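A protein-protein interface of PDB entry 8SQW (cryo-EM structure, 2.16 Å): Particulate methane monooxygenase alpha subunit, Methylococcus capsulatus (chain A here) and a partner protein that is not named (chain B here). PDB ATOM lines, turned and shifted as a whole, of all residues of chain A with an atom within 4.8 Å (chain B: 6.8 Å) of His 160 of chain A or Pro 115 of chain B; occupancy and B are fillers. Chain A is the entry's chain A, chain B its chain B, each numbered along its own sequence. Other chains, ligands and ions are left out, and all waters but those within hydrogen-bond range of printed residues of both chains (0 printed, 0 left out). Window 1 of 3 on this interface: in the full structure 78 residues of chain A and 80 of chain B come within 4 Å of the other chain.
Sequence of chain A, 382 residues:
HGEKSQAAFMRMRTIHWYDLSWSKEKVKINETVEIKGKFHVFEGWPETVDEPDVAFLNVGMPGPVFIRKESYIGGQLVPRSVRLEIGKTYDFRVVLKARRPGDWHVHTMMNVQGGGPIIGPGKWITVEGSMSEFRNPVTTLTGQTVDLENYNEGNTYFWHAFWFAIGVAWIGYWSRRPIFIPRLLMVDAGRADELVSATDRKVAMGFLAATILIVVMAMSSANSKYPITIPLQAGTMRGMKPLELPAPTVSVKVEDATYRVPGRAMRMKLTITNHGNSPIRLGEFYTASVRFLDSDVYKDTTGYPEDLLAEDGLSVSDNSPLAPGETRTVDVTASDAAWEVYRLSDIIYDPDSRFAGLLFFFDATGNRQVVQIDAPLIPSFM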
ATOM      1  N   THR A 156      -3.082 -18.435  33.439  1.00  0.00           N
ATOM      2  CA  THR A 156      -4.190 -19.069  32.732  1.00  0.00           C
ATOM      3  C   THR A 156      -3.916 -19.148  31.235  1.00  0.00           C
ATOM      4  O   THR A 156      -4.075 -20.216  30.622  1.00  0.00           O
ATOM      5  CB  THR A 156      -5.486 -18.300  32.989  1.00  0.00           C
ATOM      6  OG1 THR A 156      -5.766 -18.284  34.393  1.00  0.00           O
ATOM      7  CG2 THR A 156      -6.638 -18.949  32.253  1.00  0.00           C
ATOM      8  N   TYR A 157      -3.496 -18.031  30.639  1.00  0.00           N
ATOM      9  CA  TYR A 157      -3.175 -18.017  29.217  1.00  0.00           C
ATOM     10  C   TYR A 157      -2.080 -19.021  28.894  1.00  0.00           C
ATOM     11  O   TYR A 157      -2.175 -19.768  27.915  1.00  0.00           O
ATOM     12  CB  TYR A 157      -2.750 -16.613  28.786  1.00  0.00           C
ATOM     13  CG  TYR A 157      -3.892 -15.694  28.439  1.00  0.00           C
ATOM     14  CD1 TYR A 157      -5.039 -16.177  27.825  1.00  0.00           C
ATOM     15  CD2 TYR A 157      -3.822 -14.335  28.714  1.00  0.00           C
ATOM     16  CE1 TYR A 157      -6.080 -15.340  27.500  1.00  0.00           C
ATOM     17  CE2 TYR A 157      -4.859 -13.489  28.393  1.00  0.00           C
ATOM     18  CZ  TYR A 157      -5.986 -13.994  27.787  1.00  0.00           C
ATOM     19  OH  TYR A 157      -7.023 -13.152  27.466  1.00  0.00           O
ATOM     20  N   PHE A 158      -1.029 -19.059  29.717  1.00  0.00           N
ATOM     21  CA  PHE A 158       0.094 -19.950  29.460  1.00  0.00           C
ATOM     22  C   PHE A 158      -0.347 -21.406  29.469  1.00  0.00           C
ATOM     23  O   PHE A 158      -0.024 -22.171  28.555  1.00  0.00           O
ATOM     24  CB  PHE A 158       1.195 -19.723  30.496  1.00  0.00           C
ATOM     25  CG  PHE A 158       2.212 -20.827  30.543  1.00  0.00           C
ATOM     26  CD1 PHE A 158       3.256 -20.862  29.635  1.00  0.00           C
ATOM     27  CD2 PHE A 158       2.122 -21.833  31.491  1.00  0.00           C
ATOM     28  CE1 PHE A 158       4.190 -21.876  29.670  1.00  0.00           C
ATOM     29  CE2 PHE A 158       3.053 -22.852  31.531  1.00  0.00           C
ATOM     30  CZ  PHE A 158       4.088 -22.872  30.619  1.00  0.00           C
ATOM     31  N   TRP A 159      -1.077 -21.813  30.507  1.00  0.00           N
ATOM     32  CA  TRP A 159      -1.459 -23.219  30.605  1.00  0.00           C
ATOM     33  C   TRP A 159      -2.425 -23.615  29.496  1.00  0.00           C
ATOM     34  O   TRP A 159      -2.291 -24.697  28.902  1.00  0.00           O
ATOM     35  CB  TRP A 159      -2.056 -23.506  31.980  1.00  0.00           C
ATOM     36  CG  TRP A 159      -1.000 -23.736  33.010  1.00  0.00           C
ATOM     37  CD1 TRP A 159      -0.757 -22.981  34.118  1.00  0.00           C
ATOM     38  CD2 TRP A 159      -0.016 -24.777  33.009  1.00  0.00           C
ATOM     39  NE1 TRP A 159       0.306 -23.495  34.815  1.00  0.00           N
ATOM     40  CE2 TRP A 159       0.780 -24.598  34.156  1.00  0.00           C
ATOM     41  CE3 TRP A 159       0.263 -25.847  32.154  1.00  0.00           C
ATOM     42  CZ2 TRP A 159       1.834 -25.448  34.467  1.00  0.00           C
ATOM     43  CZ3 TRP A 159       1.311 -26.689  32.467  1.00  0.00           C
ATOM     44  CH2 TRP A 159       2.085 -26.484  33.613  1.00  0.00           C
ATOM     45  N   HIS A 160      -3.395 -22.748  29.188  1.00  0.00           N
ATOM     46  CA  HIS A 160      -4.330 -23.073  28.118  1.00  0.00           C
ATOM     47  C   HIS A 160      -3.621 -23.168  26.774  1.00  0.00           C
ATOM     48  O   HIS A 160      -3.874 -24.098  25.999  1.00  0.00           O
ATOM     49  CB  HIS A 160      -5.458 -22.045  28.072  1.00  0.00           C
ATOM     50  CG  HIS A 160      -6.644 -22.427  28.900  1.00  0.00           C
ATOM     51  ND1 HIS A 160      -7.596 -23.323  28.465  1.00  0.00           N
ATOM     52  CD2 HIS A 160      -7.023 -22.048  30.143  1.00  0.00           C
ATOM     53  CE1 HIS A 160      -8.516 -23.474  29.402  1.00  0.00           C
ATOM     54  NE2 HIS A 160      -8.191 -22.712  30.431  1.00  0.00           N
ATOM     55  N   ALA A 161      -2.708 -22.231  26.490  1.00  0.00           N
ATOM     56  CA  ALA A 161      -1.953 -22.284  25.246  1.00  0.00           C
ATOM     57  C   ALA A 161      -1.074 -23.524  25.186  1.00  0.00           C
ATOM     58  O   ALA A 161      -0.944 -24.142  24.126  1.00  0.00           O
ATOM     59  CB  ALA A 161      -1.111 -21.020  25.090  1.00  0.00           C
ATOM     60  N   PHE A 162      -0.466 -23.906  26.310  1.00  0.00           N
ATOM     61  CA  PHE A 162       0.386 -25.090  26.339  1.00  0.00           C
ATOM     62  C   PHE A 162      -0.405 -26.346  26.001  1.00  0.00           C
ATOM     63  O   PHE A 162       0.012 -27.158  25.164  1.00  0.00           O
ATOM     64  CB  PHE A 162       1.045 -25.210  27.715  1.00  0.00           C
ATOM     65  CG  PHE A 162       1.788 -26.496  27.931  1.00  0.00           C
ATOM     66  CD1 PHE A 162       3.121 -26.609  27.570  1.00  0.00           C
ATOM     67  CD2 PHE A 162       1.166 -27.587  28.522  1.00  0.00           C
ATOM     68  CE1 PHE A 162       3.812 -27.789  27.775  1.00  0.00           C
ATOM     69  CE2 PHE A 162       1.851 -28.767  28.727  1.00  0.00           C
ATOM     70  CZ  PHE A 162       3.175 -28.866  28.353  1.00  0.00           C
ATOM     71  N   TRP A 163      -1.565 -26.525  26.638  1.00  0.00           N
ATOM     72  CA  TRP A 163      -2.336 -27.737  26.379  1.00  0.00           C
ATOM     73  C   TRP A 163      -2.936 -27.726  24.977  1.00  0.00           C
ATOM     74  O   TRP A 163      -2.982 -28.765  24.302  1.00  0.00           O
ATOM     75  CB  TRP A 163      -3.411 -27.913  27.449  1.00  0.00           C
ATOM     76  CG  TRP A 163      -2.836 -28.425  28.733  1.00  0.00           C
ATOM     77  CD1 TRP A 163      -2.848 -27.801  29.944  1.00  0.00           C
ATOM     78  CD2 TRP A 163      -2.125 -29.656  28.924  1.00  0.00           C
ATOM     79  NE1 TRP A 163      -2.208 -28.573  30.880  1.00  0.00           N
ATOM     80  CE2 TRP A 163      -1.752 -29.716  30.279  1.00  0.00           C
ATOM     81  CE3 TRP A 163      -1.776 -30.718  28.080  1.00  0.00           C
ATOM     82  CZ2 TRP A 163      -1.051 -30.793  30.812  1.00  0.00           C
ATOM     83  CZ3 TRP A 163      -1.079 -31.783  28.611  1.00  0.00           C
ATOM     84  CH2 TRP A 163      -0.724 -31.814  29.963  1.00  0.00           C
ATOM     85  N   PHE A 164      -3.376 -26.555  24.507  1.00  0.00           N
ATOM     86  CA  PHE A 164      -3.855 -26.451  23.133  1.00  0.00           C
ATOM     87  C   PHE A 164      -2.750 -26.796  22.145  1.00  0.00           C
ATOM     88  O   PHE A 164      -2.996 -27.465  21.137  1.00  0.00           O
ATOM     89  CB  PHE A 164      -4.394 -25.046  22.875  1.00  0.00           C
ATOM     90  CG  PHE A 164      -5.405 -24.978  21.772  1.00  0.00           C
ATOM     91  CD1 PHE A 164      -5.005 -24.824  20.455  1.00  0.00           C
ATOM     92  CD2 PHE A 164      -6.760 -25.066  22.049  1.00  0.00           C
ATOM     93  CE1 PHE A 164      -5.934 -24.760  19.437  1.00  0.00           C
ATOM     94  CE2 PHE A 164      -7.693 -25.004  21.034  1.00  0.00           C
ATOM     95  CZ  PHE A 164      -7.279 -24.852  19.727  1.00  0.00           C
ATOM     96  N   ASP B  43     -18.229 -23.764  33.733  1.00  0.00           N
ATOM     97  CA  ASP B  43     -17.148 -23.342  32.856  1.00  0.00           C
ATOM     98  C   ASP B  43     -17.045 -21.829  32.721  1.00  0.00           C
ATOM     99  O   ASP B  43     -15.977 -21.328  32.362  1.00  0.00           O
ATOM    100  CB  ASP B  43     -17.324 -23.966  31.471  1.00  0.00           C
ATOM    101  CG  ASP B  43     -16.070 -23.869  30.626  1.00  0.00           C
ATOM    102  OD1 ASP B  43     -15.032 -24.425  31.037  1.00  0.00           O
ATOM    103  OD2 ASP B  43     -16.123 -23.229  29.555  1.00  0.00           O
ATOM    104  N   PHE B  44     -18.119 -21.095  33.005  1.00  0.00           N
ATOM    105  CA  PHE B  44     -18.120 -19.646  32.850  1.00  0.00           C
ATOM    106  C   PHE B  44     -17.368 -18.923  33.959  1.00  0.00           C
ATOM    107  O   PHE B  44     -16.751 -17.885  33.704  1.00  0.00           O
ATOM    108  CB  PHE B  44     -19.557 -19.119  32.796  1.00  0.00           C
ATOM    109  CG  PHE B  44     -20.270 -19.420  31.511  1.00  0.00           C
ATOM    110  CD1 PHE B  44     -19.571 -19.852  30.397  1.00  0.00           C
ATOM    111  CD2 PHE B  44     -21.643 -19.277  31.421  1.00  0.00           C
ATOM    112  CE1 PHE B  44     -20.228 -20.133  29.219  1.00  0.00           C
ATOM    113  CE2 PHE B  44     -22.306 -19.557  30.244  1.00  0.00           C
ATOM    114  CZ  PHE B  44     -21.598 -19.986  29.142  1.00  0.00           C
ATOM    115  N   LYS B  49     -15.954 -22.815  39.630  1.00  0.00           N
ATOM    116  CA  LYS B  49     -15.013 -23.937  39.523  1.00  0.00           C
ATOM    117  C   LYS B  49     -14.706 -24.489  40.916  1.00  0.00           C
ATOM    118  O   LYS B  49     -13.678 -24.192  41.528  1.00  0.00           O
ATOM    119  CB  LYS B  49     -13.732 -23.510  38.814  1.00  0.00           C
ATOM    120  CG  LYS B  49     -13.945 -22.647  37.593  1.00  0.00           C
ATOM    121  CD  LYS B  49     -13.774 -23.435  36.313  1.00  0.00           C
ATOM    122  CE  LYS B  49     -13.573 -22.518  35.126  1.00  0.00           C
ATOM    123  NZ  LYS B  49     -14.787 -21.703  34.867  1.00  0.00           N
ATOM    124  N   TRP B  54     -18.299 -29.046  39.798  1.00  0.00           N
ATOM    125  CA  TRP B  54     -17.519 -28.845  38.583  1.00  0.00           C
ATOM    126  C   TRP B  54     -16.763 -30.113  38.207  1.00  0.00           C
ATOM    127  O   TRP B  54     -16.902 -30.636  37.089  1.00  0.00           O
ATOM    128  CB  TRP B  54     -16.566 -27.667  38.803  1.00  0.00           C
ATOM    129  CG  TRP B  54     -15.651 -27.341  37.677  1.00  0.00           C
ATOM    130  CD1 TRP B  54     -15.993 -27.103  36.380  1.00  0.00           C
ATOM    131  CD2 TRP B  54     -14.234 -27.179  37.754  1.00  0.00           C
ATOM    132  NE1 TRP B  54     -14.874 -26.818  35.639  1.00  0.00           N
ATOM    133  CE2 TRP B  54     -13.778 -26.858  36.462  1.00  0.00           C
ATOM    134  CE3 TRP B  54     -13.302 -27.283  38.791  1.00  0.00           C
ATOM    135  CZ2 TRP B  54     -12.433 -26.640  36.178  1.00  0.00           C
ATOM    136  CZ3 TRP B  54     -11.971 -27.066  38.507  1.00  0.00           C
ATOM    137  CH2 TRP B  54     -11.548 -26.748  37.215  1.00  0.00           C
ATOM    138  N   LEU B  90     -13.981 -27.473  21.085  1.00  0.00           N
ATOM    139  CA  LEU B  90     -14.710 -26.899  22.210  1.00  0.00           C
ATOM    140  C   LEU B  90     -13.913 -25.779  22.862  1.00  0.00           C
ATOM    141  O   LEU B  90     -14.463 -24.714  23.165  1.00  0.00           O
ATOM    142  CB  LEU B  90     -15.045 -27.984  23.230  1.00  0.00           C
ATOM    143  CG  LEU B  90     -15.744 -27.500  24.501  1.00  0.00           C
ATOM    144  CD1 LEU B  90     -17.011 -26.735  24.157  1.00  0.00           C
ATOM    145  CD2 LEU B  90     -16.051 -28.666  25.423  1.00  0.00           C
ATOM    146  N   LEU B  91     -12.615 -25.999  23.074  1.00  0.00           N
ATOM    147  CA  LEU B  91     -11.779 -24.976  23.695  1.00  0.00           C
ATOM    148  C   LEU B  91     -11.670 -23.743  22.813  1.00  0.00           C
ATOM    149  O   LEU B  91     -11.686 -22.616  23.314  1.00  0.00           O
ATOM    150  CB  LEU B  91     -10.394 -25.545  23.996  1.00  0.00           C
ATOM    151  CG  LEU B  91     -10.284 -26.375  25.275  1.00  0.00           C
ATOM    152  CD1 LEU B  91      -9.008 -27.192  25.272  1.00  0.00           C
ATOM    153  CD2 LEU B  91     -10.341 -25.477  26.495  1.00  0.00           C
ATOM    154  N   GLU B  94     -15.028 -21.876  22.997  1.00  0.00           N
ATOM    155  CA  GLU B  94     -15.179 -21.291  24.320  1.00  0.00           C
ATOM    156  C   GLU B  94     -14.269 -20.084  24.490  1.00  0.00           C
ATOM    157  O   GLU B  94     -14.701 -19.040  24.980  1.00  0.00           O
ATOM    158  CB  GLU B  94     -14.893 -22.345  25.389  1.00  0.00           C
ATOM    159  CG  GLU B  94     -16.070 -23.258  25.680  1.00  0.00           C
ATOM    160  CD  GLU B  94     -15.710 -24.402  26.604  1.00  0.00           C
ATOM    161  OE1 GLU B  94     -14.539 -24.833  26.591  1.00  0.00           O
ATOM    162  OE2 GLU B  94     -16.601 -24.877  27.338  1.00  0.00           O
ATOM    163  N   TRP B  95     -13.004 -20.201  24.079  1.00  0.00           N
ATOM    164  CA  TRP B  95     -12.066 -19.095  24.228  1.00  0.00           C
ATOM    165  C   TRP B  95     -12.438 -17.918  23.343  1.00  0.00           C
ATOM    166  O   TRP B  95     -12.313 -16.762  23.766  1.00  0.00           O
ATOM    167  CB  TRP B  95     -10.642 -19.557  23.921  1.00  0.00           C
ATOM    168  CG  TRP B  95      -9.868 -19.931  25.141  1.00  0.00           C
ATOM    169  CD1 TRP B  95      -9.425 -21.173  25.480  1.00  0.00           C
ATOM    170  CD2 TRP B  95      -9.454 -19.055  26.194  1.00  0.00           C
ATOM    171  NE1 TRP B  95      -8.755 -21.126  26.677  1.00  0.00           N
ATOM    172  CE2 TRP B  95      -8.757 -19.836  27.136  1.00  0.00           C
ATOM    173  CE3 TRP B  95      -9.598 -17.684  26.431  1.00  0.00           C
ATOM    174  CZ2 TRP B  95      -8.211 -19.295  28.295  1.00  0.00           C
ATOM    175  CZ3 TRP B  95      -9.054 -17.150  27.581  1.00  0.00           C
ATOM    176  CH2 TRP B  95      -8.370 -17.954  28.500  1.00  0.00           C
ATOM    177  N   ARG B  98     -15.258 -16.258  25.150  1.00  0.00           N
ATOM    178  CA  ARG B  98     -14.783 -15.602  26.365  1.00  0.00           C
ATOM    179  C   ARG B  98     -14.084 -14.292  26.038  1.00  0.00           C
ATOM    180  O   ARG B  98     -14.333 -13.268  26.685  1.00  0.00           O
ATOM    181  CB  ARG B  98     -13.820 -16.510  27.134  1.00  0.00           C
ATOM    182  CG  ARG B  98     -14.387 -17.807  27.676  1.00  0.00           C
ATOM    183  CD  ARG B  98     -15.808 -17.685  28.157  1.00  0.00           C
ATOM    184  NE  ARG B  98     -16.524 -18.942  27.979  1.00  0.00           N
ATOM    185  CZ  ARG B  98     -16.448 -19.972  28.809  1.00  0.00           C
ATOM    186  NH1 ARG B  98     -15.695 -19.928  29.898  1.00  0.00           N
ATOM    187  NH2 ARG B  98     -17.136 -21.076  28.540  1.00  0.00           N
ATOM    188  N   ILE B 110     -10.666 -11.876  31.965  1.00  0.00           N
ATOM    189  CA  ILE B 110     -10.368 -13.216  31.471  1.00  0.00           C
ATOM    190  C   ILE B 110     -10.029 -14.149  32.627  1.00  0.00           C
ATOM    191  O   ILE B 110     -10.417 -15.323  32.628  1.00  0.00           O
ATOM    192  CB  ILE B 110      -9.233 -13.156  30.432  1.00  0.00           C
ATOM    193  CG1 ILE B 110      -9.688 -12.366  29.204  1.00  0.00           C
ATOM    194  CG2 ILE B 110      -8.773 -14.553  30.046  1.00  0.00           C
ATOM    195  CD1 ILE B 110     -10.509 -13.168  28.223  1.00  0.00           C
ATOM    196  N   VAL B 113     -13.383 -15.339  33.673  1.00  0.00           N
ATOM    197  CA  VAL B 113     -14.258 -16.082  32.770  1.00  0.00           C
ATOM    198  C   VAL B 113     -13.490 -17.099  31.922  1.00  0.00           C
ATOM    199  O   VAL B 113     -13.975 -17.513  30.874  1.00  0.00           O
ATOM    200  CB  VAL B 113     -15.076 -15.133  31.882  1.00  0.00           C
ATOM    201  CG1 VAL B 113     -16.015 -14.300  32.730  1.00  0.00           C
ATOM    202  CG2 VAL B 113     -14.159 -14.246  31.055  1.00  0.00           C
ATOM    203  N   PHE B 114     -12.306 -17.521  32.359  1.00  0.00           N
ATOM    204  CA  PHE B 114     -11.549 -18.503  31.596  1.00  0.00           C
ATOM    205  C   PHE B 114     -12.258 -19.861  31.596  1.00  0.00           C
ATOM    206  O   PHE B 114     -12.940 -20.214  32.558  1.00  0.00           O
ATOM    207  CB  PHE B 114     -10.147 -18.658  32.170  1.00  0.00           C
ATOM    208  CG  PHE B 114     -10.123 -19.153  33.585  1.00  0.00           C
ATOM    209  CD1 PHE B 114     -10.191 -18.263  34.641  1.00  0.00           C
ATOM    210  CD2 PHE B 114     -10.033 -20.507  33.859  1.00  0.00           C
ATOM    211  CE1 PHE B 114     -10.175 -18.716  35.942  1.00  0.00           C
ATOM    212  CE2 PHE B 114     -10.016 -20.963  35.159  1.00  0.00           C
ATOM    213  CZ  PHE B 114     -10.086 -20.065  36.202  1.00  0.00           C
ATOM    214  N   PRO B 115     -12.108 -20.639  30.531  1.00  0.00           N
ATOM    215  CA  PRO B 115     -12.670 -21.993  30.492  1.00  0.00           C
ATOM    216  C   PRO B 115     -11.733 -22.997  31.160  1.00  0.00           C
ATOM    217  O   PRO B 115     -10.598 -22.694  31.516  1.00  0.00           O
ATOM    218  CB  PRO B 115     -12.805 -22.267  28.995  1.00  0.00           C
ATOM    219  CG  PRO B 115     -11.716 -21.467  28.383  1.00  0.00           C
ATOM    220  CD  PRO B 115     -11.553 -20.235  29.228  1.00  0.00           C
ATOM    221  N   ALA B 116     -12.242 -24.215  31.329  1.00  0.00           N
ATOM    222  CA  ALA B 116     -11.474 -25.316  31.895  1.00  0.00           C
ATOM    223  C   ALA B 116     -10.600 -25.969  30.832  1.00  0.00           C
ATOM    224  O   ALA B 116     -10.841 -25.838  29.631  1.00  0.00           O
ATOM    225  CB  ALA B 116     -12.403 -26.359  32.516  1.00  0.00           C
ATOM    226  N   SER B 117      -9.570 -26.680  31.293  1.00  0.00           N
ATOM    227  CA  SER B 117      -8.654 -27.396  30.415  1.00  0.00           C
ATOM    228  C   SER B 117      -9.083 -28.857  30.297  1.00  0.00           C
ATOM    229  O   SER B 117      -9.449 -29.484  31.296  1.00  0.00           O
ATOM    230  CB  SER B 117      -7.223 -27.301  30.945  1.00  0.00           C
ATOM    231  OG  SER B 117      -6.311 -27.946  30.076  1.00  0.00           O
ATOM    232  N   LEU B 118      -9.037 -29.395  29.070  1.00  0.00           N
ATOM    233  CA  LEU B 118      -9.513 -30.747  28.790  1.00  0.00           C
ATOM    234  C   LEU B 118      -8.554 -31.548  27.912  1.00  0.00           C
ATOM    235  O   LEU B 118      -8.785 -32.751  27.690  1.00  0.00           O
ATOM    236  CB  LEU B 118     -10.890 -30.695  28.126  1.00  0.00           C
ATOM    237  CG  LEU B 118     -11.905 -29.770  28.793  1.00  0.00           C
ATOM    238  CD1 LEU B 118     -12.818 -29.134  27.756  1.00  0.00           C
ATOM    239  CD2 LEU B 118     -12.689 -30.518  29.854  1.00  0.00           C
ATOM    240  N   VAL B 119      -7.502 -30.911  27.398  1.00  0.00           N
ATOM    241  CA  VAL B 119      -6.577 -31.604  26.501  1.00  0.00           C
ATOM    242  C   VAL B 119      -5.936 -32.830  27.144  1.00  0.00           C
ATOM    243  O   VAL B 119      -5.764 -33.841  26.446  1.00  0.00           O
ATOM    244  CB  VAL B 119      -5.534 -30.616  25.950  1.00  0.00           C
ATOM    245  CG1 VAL B 119      -4.423 -31.362  25.228  1.00  0.00           C
ATOM    246  CG2 VAL B 119      -6.196 -29.624  25.015  1.00  0.00           C
ATOM    247  N   ASN B 154      -6.483 -29.007  35.743  1.00  0.00           N
ATOM    248  CA  ASN B 154      -6.876 -27.617  35.913  1.00  0.00           C
ATOM    249  C   ASN B 154      -6.333 -26.986  37.185  1.00  0.00           C
ATOM    250  O   ASN B 154      -6.465 -25.771  37.360  1.00  0.00           O
ATOM    251  CB  ASN B 154      -8.402 -27.491  35.905  1.00  0.00           C
ATOM    252  CG  ASN B 154      -8.992 -27.679  34.526  1.00  0.00           C
ATOM    253  OD1 ASN B 154      -9.056 -26.740  33.734  1.00  0.00           O
ATOM    254  ND2 ASN B 154      -9.436 -28.894  34.234  1.00  0.00           N
ATOM    255  N   ILE B 157      -4.075 -23.848  37.014  1.00  0.00           N
ATOM    256  CA  ILE B 157      -4.752 -22.617  36.620  1.00  0.00           C
ATOM    257  C   ILE B 157      -5.519 -22.015  37.791  1.00  0.00           C
ATOM    258  O   ILE B 157      -5.438 -20.810  38.050  1.00  0.00           O
ATOM    259  CB  ILE B 157      -5.678 -22.879  35.418  1.00  0.00           C
ATOM    260  CG1 ILE B 157      -4.869 -23.390  34.224  1.00  0.00           C
ATOM    261  CG2 ILE B 157      -6.439 -21.623  35.043  1.00  0.00           C
ATOM    262  CD1 ILE B 157      -5.660 -24.270  33.288  1.00  0.00           C
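NE1 of Trp 95 of chain B is in hydrogen-bond range of ND1 of His 160 of chain A, at 3.1 Å. NE2 of His 160 of chain A is in hydrogen-bond range of O of Pro 115 of chain B (2.6 Å).
The side-chain carboxylate (OD1) of Asp 43 of chain B sits at hydrogen-bond distance from the backbone NH (N) of Ala 116 of chain B, 2.8 Å away. The side-chain amino group (NZ) of Lys 49 of chain B lies within hydrogen-bond range of the backbone carbonyl oxygen (O) of Phe 114 of chain B, 3.3 Å away. The backbone NH (N) of Ser 117 of chain B sits at hydrogen-bond distance from the side-chain amide oxygen (OD1) of Asn 154 of chain B (2.5 Å).
Among the printed residues, merely in contact across the chains: Trp 163 of chain A with Val 119 of chain B, Tyr 157 of chain A with Ile 110 of chain B, His 160 of chain A with Ala 116 of chain B, Thr 156 of chain A with Ile 157 of chain B, Trp 163 of chain A with Ser 117 of chain B, Tyr 157 of chain A with Trp 95 of chain B, Thr 156 of chain A with Phe 114 of chain B, Trp 159 of chain A with Ile 157 of chain B, His 160 of chain A with Ser 117 of chain B and His 160 of chain A with Leu 91 of chain B.
Of the printed residues of chain B, Tyr 157 of chain A touches Trp 95 and Ile 110. Of chain B, only Leu 91 (3.97 Å), Trp 95 (3.1 Å), Pro 115 (2.6 Å), Ala 116 (3.3 Å) and Ser 117 (3.9 Å) come within 4 Å of His 160 of chain A. Lys 49 of chain B touches none of the printed residues of chain A. Of the printed residues of chain A, Leu 91 of chain B touches His 160 (3.97 Å). Of the printed residues of chain A, Trp 95 of chain B touches Tyr 157 and His 160. Of the printed residues of chain A, Phe 114 of chain B touches Thr 156. Pro 115 of chain B touches one residue of chain A. Printed residues of chain A within 4 Å of Val 119 of chain B: Trp 163 (3.1 Å). The nearest printed residue of chain A that does not touch Pro 115 of chain B is Thr 156 of chain A (5.5 Å).
Printed residues of chain A that touch a printed residue of chain B: Thr 156, Tyr 157, Trp 159, His 160 and Trp 163. Hydrophobic or aromatic side chains of chain A that line the printed part of chain B: Tyr 157, Trp 159, His 160 and Trp 163. Printed residues of chain B that touch a printed residue of chain A: Leu 91, Trp 95, Ile 110, Phe 114, Pro 115, Ala 116, Ser 117, Val 119 and Ile 157. Hydrophobic or aromatic side chains of chain B within 4 Å of the printed part of chain A: Leu 91, Trp 95, Ile 110, Phe 114, Pro 115, Val 119 and Ile 157.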
